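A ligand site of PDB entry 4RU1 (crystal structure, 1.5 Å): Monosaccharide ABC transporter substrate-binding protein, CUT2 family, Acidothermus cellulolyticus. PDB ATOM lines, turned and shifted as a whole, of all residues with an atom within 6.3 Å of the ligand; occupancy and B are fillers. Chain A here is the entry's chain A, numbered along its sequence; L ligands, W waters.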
ATOM      1  N   HIS A  28      23.144   0.501  18.671  1.00  0.00           N
ATOM      2  CA  HIS A  28      21.740   0.514  19.089  1.00  0.00           C
ATOM      3  C   HIS A  28      20.784   1.164  18.093  1.00  0.00           C
ATOM      4  O   HIS A  28      19.665   1.446  18.467  1.00  0.00           O
ATOM      5  CB  HIS A  28      21.645   1.226  20.433  1.00  0.00           C
ATOM      6  CG  HIS A  28      22.114   2.663  20.383  1.00  0.00           C
ATOM      7  ND1 HIS A  28      23.449   2.993  20.599  1.00  0.00           N
ATOM      8  CD2 HIS A  28      21.463   3.823  20.188  1.00  0.00           C
ATOM      9  CE1 HIS A  28      23.582   4.300  20.537  1.00  0.00           C
ATOM     10  NE2 HIS A  28      22.404   4.820  20.270  1.00  0.00           N
ATOM     11  N   GLN A  29      21.267   1.392  16.849  1.00  0.00           N
ATOM     12  CA  GLN A  29      20.545   2.054  15.764  1.00  0.00           C
ATOM     13  C   GLN A  29      19.116   1.474  15.674  1.00  0.00           C
ATOM     14  O   GLN A  29      18.945   0.227  15.555  1.00  0.00           O
ATOM     15  CB  GLN A  29      21.283   1.880  14.467  1.00  0.00           C
ATOM     16  CG  GLN A  29      20.460   2.263  13.271  1.00  0.00           C
ATOM     17  CD  GLN A  29      21.159   2.125  11.981  1.00  0.00           C
ATOM     18  OE1 GLN A  29      22.182   1.467  11.867  1.00  0.00           O
ATOM     19  NE2 GLN A  29      20.638   2.788  10.969  1.00  0.00           N
ATOM     20  N   GLN A  30      18.144   2.360  15.758  1.00  0.00           N
ATOM     21  CA  GLN A  30      16.775   2.006  15.352  1.00  0.00           C
ATOM     22  C   GLN A  30      16.738   1.938  13.852  1.00  0.00           C
ATOM     23  O   GLN A  30      17.221   2.867  13.164  1.00  0.00           O
ATOM     24  CB  GLN A  30      15.811   3.067  15.815  1.00  0.00           C
ATOM     25  CG  GLN A  30      14.386   2.880  15.374  1.00  0.00           C
ATOM     26  CD  GLN A  30      13.681   1.827  16.217  1.00  0.00           C
ATOM     27  OE1 GLN A  30      13.841   1.742  17.437  1.00  0.00           O
ATOM     28  NE2 GLN A  30      12.898   1.006  15.563  1.00  0.00           N
ATOM     29  N   ASP A  33      16.948   5.217  11.281  1.00  0.00           N
ATOM     30  CA  ASP A  33      17.563   6.395  11.908  1.00  0.00           C
ATOM     31  C   ASP A  33      18.818   6.744  11.099  1.00  0.00           C
ATOM     32  O   ASP A  33      19.884   6.094  11.204  1.00  0.00           O
ATOM     33  CB  ASP A  33      17.832   6.134  13.373  1.00  0.00           C
ATOM     34  CG  ASP A  33      18.463   7.365  14.067  1.00  0.00           C
ATOM     35  OD1 ASP A  33      18.710   8.360  13.335  1.00  0.00           O
ATOM     36  OD2 ASP A  33      18.678   7.294  15.309  1.00  0.00           O
ATOM     37  N   PHE A  35      20.923   9.047  11.186  1.00  0.00           N
ATOM     38  CA  PHE A  35      22.140   9.487  11.873  1.00  0.00           C
ATOM     39  C   PHE A  35      23.241   8.481  11.702  1.00  0.00           C
ATOM     40  O   PHE A  35      24.365   8.826  11.485  1.00  0.00           O
ATOM     41  CB  PHE A  35      21.883   9.653  13.368  1.00  0.00           C
ATOM     42  CG  PHE A  35      23.127   9.848  14.179  1.00  0.00           C
ATOM     43  CD1 PHE A  35      23.701  11.070  14.289  1.00  0.00           C
ATOM     44  CD2 PHE A  35      23.633   8.798  14.934  1.00  0.00           C
ATOM     45  CE1 PHE A  35      24.825  11.252  15.108  1.00  0.00           C
ATOM     46  CE2 PHE A  35      24.734   8.950  15.720  1.00  0.00           C
ATOM     47  CZ  PHE A  35      25.341  10.186  15.775  1.00  0.00           C
ATOM     48  N   TRP A  36      22.883   7.214  11.716  1.00  0.00           N
ATOM     49  CA  TRP A  36      23.824   6.076  11.808  1.00  0.00           C
ATOM     50  C   TRP A  36      24.460   5.902  10.400  1.00  0.00           C
ATOM     51  O   TRP A  36      25.515   5.269  10.262  1.00  0.00           O
ATOM     52  CB  TRP A  36      23.127   4.816  12.342  1.00  0.00           C
ATOM     53  CG  TRP A  36      22.833   5.000  13.752  1.00  0.00           C
ATOM     54  CD1 TRP A  36      21.639   5.499  14.312  1.00  0.00           C
ATOM     55  CD2 TRP A  36      23.759   4.924  14.828  1.00  0.00           C
ATOM     56  NE1 TRP A  36      21.803   5.675  15.692  1.00  0.00           N
ATOM     57  CE2 TRP A  36      23.093   5.347  16.002  1.00  0.00           C
ATOM     58  CE3 TRP A  36      25.120   4.529  14.917  1.00  0.00           C
ATOM     59  CZ2 TRP A  36      23.761   5.349  17.239  1.00  0.00           C
ATOM     60  CZ3 TRP A  36      25.726   4.552  16.145  1.00  0.00           C
ATOM     61  CH2 TRP A  36      25.085   4.984  17.260  1.00  0.00           C
ATOM     62  N   ASN A 108      29.949   6.875  20.886  1.00  0.00           N
ATOM     63  CA  ASN A 108      28.635   7.463  20.723  1.00  0.00           C
ATOM     64  C   ASN A 108      27.779   7.508  22.026  1.00  0.00           C
ATOM     65  O   ASN A 108      27.253   8.573  22.363  1.00  0.00           O
ATOM     66  CB  ASN A 108      27.810   6.829  19.657  1.00  0.00           C
ATOM     67  CG  ASN A 108      26.498   7.527  19.488  1.00  0.00           C
ATOM     68  OD1 ASN A 108      25.474   7.038  19.976  1.00  0.00           O
ATOM     69  ND2 ASN A 108      26.474   8.657  18.845  1.00  0.00           N
ATOM     70  N   ALA A 109      27.636   6.370  22.713  1.00  0.00           N
ATOM     71  CA  ALA A 109      26.897   6.310  23.953  1.00  0.00           C
ATOM     72  C   ALA A 109      27.671   5.583  24.990  1.00  0.00           C
ATOM     73  O   ALA A 109      28.217   4.545  24.701  1.00  0.00           O
ATOM     74  CB  ALA A 109      25.568   5.669  23.760  1.00  0.00           C
ATOM     75  N   GLU A 127      27.730  14.327  26.827  1.00  0.00           N
ATOM     76  CA  GLU A 127      26.372  14.719  26.583  1.00  0.00           C
ATOM     77  C   GLU A 127      25.779  15.605  27.717  1.00  0.00           C
ATOM     78  O   GLU A 127      24.922  16.457  27.464  1.00  0.00           O
ATOM     79  CB  GLU A 127      25.470  13.512  26.317  1.00  0.00           C
ATOM     80  CG  GLU A 127      25.824  12.691  25.072  1.00  0.00           C
ATOM     81  CD  GLU A 127      25.716  13.433  23.737  1.00  0.00           C
ATOM     82  OE1 GLU A 127      25.402  14.635  23.705  1.00  0.00           O
ATOM     83  OE2 GLU A 127      25.985  12.774  22.708  1.00  0.00           O
ATOM     84  N   GLN A 151      13.507  10.698  21.762  1.00  0.00           N
ATOM     85  CA  GLN A 151      12.917   9.733  20.875  1.00  0.00           C
ATOM     86  C   GLN A 151      12.996   8.301  21.325  1.00  0.00           C
ATOM     87  O   GLN A 151      12.575   7.410  20.564  1.00  0.00           O
ATOM     88  CB  GLN A 151      13.434   9.910  19.472  1.00  0.00           C
ATOM     89  CG  GLN A 151      14.894   9.492  19.260  1.00  0.00           C
ATOM     90  CD  GLN A 151      15.946  10.569  19.538  1.00  0.00           C
ATOM     91  OE1 GLN A 151      15.742  11.541  20.264  1.00  0.00           O
ATOM     92  NE2 GLN A 151      17.125  10.380  18.990  1.00  0.00           N
ATOM     93  N   GLN A 155      17.904   5.522  27.487  1.00  0.00           N
ATOM     94  CA  GLN A 155      19.174   5.640  26.786  1.00  0.00           C
ATOM     95  C   GLN A 155      20.049   6.733  27.444  1.00  0.00           C
ATOM     96  O   GLN A 155      19.652   7.927  27.437  1.00  0.00           O
ATOM     97  CB  GLN A 155      18.957   5.916  25.314  1.00  0.00           C
ATOM     98  CG  GLN A 155      18.435   4.672  24.611  1.00  0.00           C
ATOM     99  CD  GLN A 155      18.484   4.709  23.130  1.00  0.00           C
ATOM    100  OE1 GLN A 155      19.119   5.527  22.495  1.00  0.00           O
ATOM    101  NE2 GLN A 155      17.797   3.776  22.525  1.00  0.00           N
ATOM    102  N   GLN A 157      22.672   8.361  26.891  1.00  0.00           N
ATOM    103  CA  GLN A 157      23.194   9.503  26.124  1.00  0.00           C
ATOM    104  C   GLN A 157      22.126  10.560  25.855  1.00  0.00           C
ATOM    105  O   GLN A 157      22.436  11.771  25.745  1.00  0.00           O
ATOM    106  CB  GLN A 157      23.867   9.107  24.817  1.00  0.00           C
ATOM    107  CG  GLN A 157      22.942   8.713  23.656  1.00  0.00           C
ATOM    108  CD  GLN A 157      22.219   7.373  23.790  1.00  0.00           C
ATOM    109  OE1 GLN A 157      22.281   6.667  24.783  1.00  0.00           O
ATOM    110  NE2 GLN A 157      21.611   7.017  22.675  1.00  0.00           N
ATOM    111  N   LEU A 158      20.885  10.132  25.757  1.00  0.00           N
ATOM    112  CA  LEU A 158      19.761  11.029  25.589  1.00  0.00           C
ATOM    113  C   LEU A 158      19.384  11.633  26.938  1.00  0.00           C
ATOM    114  O   LEU A 158      19.175  12.883  27.012  1.00  0.00           O
ATOM    115  CB  LEU A 158      18.571  10.283  24.960  1.00  0.00           C
ATOM    116  CG  LEU A 158      18.795   9.712  23.556  1.00  0.00           C
ATOM    117  CD1 LEU A 158      17.520   9.104  23.028  1.00  0.00           C
ATOM    118  CD2 LEU A 158      19.442  10.736  22.606  1.00  0.00           C
ATOM    119  N   ARG A 161      21.659  14.450  28.012  1.00  0.00           N
ATOM    120  CA  ARG A 161      21.434  15.713  27.340  1.00  0.00           C
ATOM    121  C   ARG A 161      20.330  16.530  28.032  1.00  0.00           C
ATOM    122  O   ARG A 161      20.524  17.700  28.360  1.00  0.00           O
ATOM    123  CB  ARG A 161      21.055  15.509  25.856  1.00  0.00           C
ATOM    124  CG  ARG A 161      22.142  14.955  24.981  1.00  0.00           C
ATOM    125  CD  ARG A 161      21.699  14.743  23.533  1.00  0.00           C
ATOM    126  NE  ARG A 161      22.830  14.244  22.738  1.00  0.00           N
ATOM    127  CZ  ARG A 161      22.701  13.704  21.538  1.00  0.00           C
ATOM    128  NH1 ARG A 161      21.537  13.654  20.901  1.00  0.00           N
ATOM    129  NH2 ARG A 161      23.754  13.331  20.908  1.00  0.00           N
ATOM    130  N   LEU A 206      16.566  15.903  19.947  1.00  0.00           N
ATOM    131  CA  LEU A 206      17.798  15.144  20.204  1.00  0.00           C
ATOM    132  C   LEU A 206      18.348  14.393  18.957  1.00  0.00           C
ATOM    133  O   LEU A 206      19.317  13.578  19.050  1.00  0.00           O
ATOM    134  CB  LEU A 206      17.698  14.238  21.370  1.00  0.00           C
ATOM    135  CG  LEU A 206      17.237  14.885  22.644  1.00  0.00           C
ATOM    136  CD1 LEU A 206      17.307  13.913  23.818  1.00  0.00           C
ATOM    137  CD2 LEU A 206      17.824  16.190  23.011  1.00  0.00           C
ATOM    138  N   GLY A 207      17.752  14.661  17.793  1.00  0.00           N
ATOM    139  CA  GLY A 207      18.254  14.209  16.533  1.00  0.00           C
ATOM    140  C   GLY A 207      17.676  15.016  15.408  1.00  0.00           C
ATOM    141  O   GLY A 207      16.551  15.581  15.538  1.00  0.00           O
ATOM    142  N   ALA A 208      18.397  15.043  14.312  1.00  0.00           N
ATOM    143  CA  ALA A 208      17.978  15.847  13.145  1.00  0.00           C
ATOM    144  C   ALA A 208      16.656  15.397  12.485  1.00  0.00           C
ATOM    145  O   ALA A 208      15.872  16.237  12.083  1.00  0.00           O
ATOM    146  CB  ALA A 208      19.124  15.894  12.130  1.00  0.00           C
ATOM    147  N   PHE A 230      20.067  18.741  18.319  1.00  0.00           N
ATOM    148  CA  PHE A 230      21.319  18.043  18.202  1.00  0.00           C
ATOM    149  C   PHE A 230      21.411  17.478  16.786  1.00  0.00           C
ATOM    150  O   PHE A 230      20.386  16.907  16.267  1.00  0.00           O
ATOM    151  CB  PHE A 230      21.400  16.935  19.260  1.00  0.00           C
ATOM    152  CG  PHE A 230      21.598  17.413  20.646  1.00  0.00           C
ATOM    153  CD1 PHE A 230      20.593  18.044  21.371  1.00  0.00           C
ATOM    154  CD2 PHE A 230      22.801  17.219  21.254  1.00  0.00           C
ATOM    155  CE1 PHE A 230      20.834  18.477  22.638  1.00  0.00           C
ATOM    156  CE2 PHE A 230      23.061  17.671  22.507  1.00  0.00           C
ATOM    157  CZ  PHE A 230      22.082  18.280  23.248  1.00  0.00           C
ATOM    158  N   ASP A 231      22.608  17.545  16.170  1.00  0.00           N
ATOM    159  CA  ASP A 231      22.993  16.856  14.909  1.00  0.00           C
ATOM    160  C   ASP A 231      22.554  17.553  13.656  1.00  0.00           C
ATOM    161  O   ASP A 231      21.643  18.379  13.615  1.00  0.00           O
ATOM    162  CB  ASP A 231      22.416  15.401  14.858  1.00  0.00           C
ATOM    163  CG  ASP A 231      22.799  14.542  16.027  1.00  0.00           C
ATOM    164  OD1 ASP A 231      23.900  14.712  16.603  1.00  0.00           O
ATOM    165  OD2 ASP A 231      22.020  13.625  16.381  1.00  0.00           O
ATOM    166  N   GLN A 251      28.157  16.700  16.906  1.00  0.00           N
ATOM    167  CA  GLN A 251      28.960  15.686  17.593  1.00  0.00           C
ATOM    168  C   GLN A 251      29.908  14.944  16.684  1.00  0.00           C
ATOM    169  O   GLN A 251      30.629  14.031  17.139  1.00  0.00           O
ATOM    170  CB  GLN A 251      28.120  14.661  18.368  1.00  0.00           C
ATOM    171  CG  GLN A 251      27.300  13.743  17.479  1.00  0.00           C
ATOM    172  CD  GLN A 251      26.545  12.656  18.237  1.00  0.00           C
ATOM    173  OE1 GLN A 251      25.280  12.549  18.165  1.00  0.00           O
ATOM    174  NE2 GLN A 251      27.293  11.801  18.895  1.00  0.00           N
ATOM    175  N   GLU A 256      33.333   9.976  14.975  1.00  0.00           N
ATOM    176  CA  GLU A 256      33.065   8.851  15.874  1.00  0.00           C
ATOM    177  C   GLU A 256      33.243   7.490  15.193  1.00  0.00           C
ATOM    178  O   GLU A 256      33.965   6.631  15.718  1.00  0.00           O
ATOM    179  CB  GLU A 256      31.675   8.928  16.457  1.00  0.00           C
ATOM    180  CG  GLU A 256      31.455  10.190  17.300  1.00  0.00           C
ATOM    181  CD  GLU A 256      30.078  10.319  17.882  1.00  0.00           C
ATOM    182  OE1 GLU A 256      29.210   9.420  17.762  1.00  0.00           O
ATOM    183  OE2 GLU A 256      29.781  11.408  18.465  1.00  0.00           O
HETATM  184  C1  LIG L   1      22.108  10.945  18.206  1.00  0.00           C
HETATM  185  C2  LIG L   1      20.683  10.672  17.768  1.00  0.00           C
HETATM  186  C3  LIG L   1      20.519   9.177  17.473  1.00  0.00           C
HETATM  187  C4  LIG L   1      21.018   8.290  18.594  1.00  0.00           C
HETATM  188  C5  LIG L   1      22.446   8.568  18.938  1.00  0.00           C
HETATM  189  C6  LIG L   1      22.703  10.015  19.250  1.00  0.00           C
HETATM  190  O1  LIG L   1      22.326  12.316  18.561  1.00  0.00           O
HETATM  191  O2  LIG L   1      19.865  10.961  18.918  1.00  0.00           O
HETATM  192  O3  LIG L   1      19.106   8.974  17.274  1.00  0.00           O
HETATM  193  O4  LIG L   1      20.839   6.895  18.251  1.00  0.00           O
HETATM  194  O5  LIG L   1      22.894   7.818  20.085  1.00  0.00           O
HETATM  195  O6  LIG L   1      24.130  10.263  19.454  1.00  0.00           O
HETATM  196  O   HOH W   1      18.655   4.953  16.754  1.00  0.00           O
HETATM  197  O   HOH W   2      18.755  10.704  14.909  1.00  0.00           O
HETATM  198  O   HOH W   3      25.099  10.304  21.909  1.00  0.00           O
HETATM  199  O   HOH W   4      18.694   6.304  20.043  1.00  0.00           O
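An oxygen (O2) of the ligand sits at hydrogen-bond distance from the backbone carbonyl oxygen of Leu 206 (2.7 Å).
NE2 of Gln 151 lies within hydrogen-bond range of O2 of the ligand (2.8 Å).
OD2 of Asp 231 sits at hydrogen-bond distance from O1 of the ligand, 2.6 Å away.
The side-chain amide nitrogen of Gln 157 lies within hydrogen-bond range of an oxygen (O5) of the ligand.
The guanidinium group of Arg 161 sits at hydrogen-bond distance from an oxygen (O1) of the ligand.
NE1 of Trp 36 is in hydrogen-bond range of O4 of the ligand (3.0 Å).
The side-chain amide oxygen of Asn 108 sits at hydrogen-bond distance from an oxygen (O5) of the ligand (2.7 Å).
An oxygen (O6) of the ligand is in hydrogen-bond range of the side-chain amide oxygen of Gln 251, at 2.9 Å.
The side-chain carboxylate (OD2) of Asp 33 sits at hydrogen-bond distance from an oxygen (O3) of the ligand (2.6 Å).
A ring nitrogen (NE2) of His 28 sits at hydrogen-bond distance from an oxygen (O5) of the ligand, at 3.0 Å.
NE of Arg 161 is in salt-bridge range of OE1 of Glu 127 (2.8 Å).
ND2 of Asn 108 lies close to NE2 of Gln 251, 3.2 Å away.
The guanidinium group of Arg 161 is in hydrogen-bond range of the backbone carbonyl oxygen of Leu 206.
The side-chain amide oxygen of Gln 251 sits close to the side-chain carboxylate of Asp 231 (3.0 Å).
The side-chain amide nitrogen of Gln 251 sits at hydrogen-bond distance from the side-chain carboxylate of Glu 256 (2.6 Å).
OD1 of Asp 33 lies close to N of Phe 35, 3.2 Å away.
O of Asp 33 lies within hydrogen-bond range of NE2 of Gln 29 (3.4 Å).
The side-chain amide nitrogen of Asn 108 sits at hydrogen-bond distance from the side-chain carboxylate of Glu 256, at 3.0 Å.
Phe 35 touches the ligand.
CD2 of Leu 158 touches O2 of the ligand, 3.7 Å away.
Hydrophobic or aromatic side chains that line the ligand: His 28, Phe 35, Trp 36 and Leu 158.
Within 4 Å of the ligand: His 28, Asp 33, Phe 35, Trp 36, Asn 108, Gln 151, Gln 157, Leu 158, Arg 161, Leu 206, Asp 231 and Gln 251.
The nearest printed residue that does not touch the ligand is Gly 207 (4.3 Å).
Water W3 lies within hydrogen-bond range of an oxygen (O6) of the ligand (2.6 Å), the side-chain carboxylate of Glu 127 (2.7 Å), the backbone carbonyl oxygen of Asn 108 (2.8 Å) and the guanidinium group of Arg 161 (3.5 Å).
Water W4 bridges the side-chain amide oxygen (OE1) of Gln 155 (2.6 Å) and an oxygen (O4) of the ligand (2.9 Å).
Water W2 bridges OD1 of Asp 33 (2.8 Å) and O3 of the ligand (3.0 Å).
Water W1 lies within hydrogen-bond range of OD2 of Asp 33 (2.8 Å), N of Gln 30 (2.8 Å), O4 of the ligand (3.3 Å) and NE1 of Trp 36 (3.4 Å).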
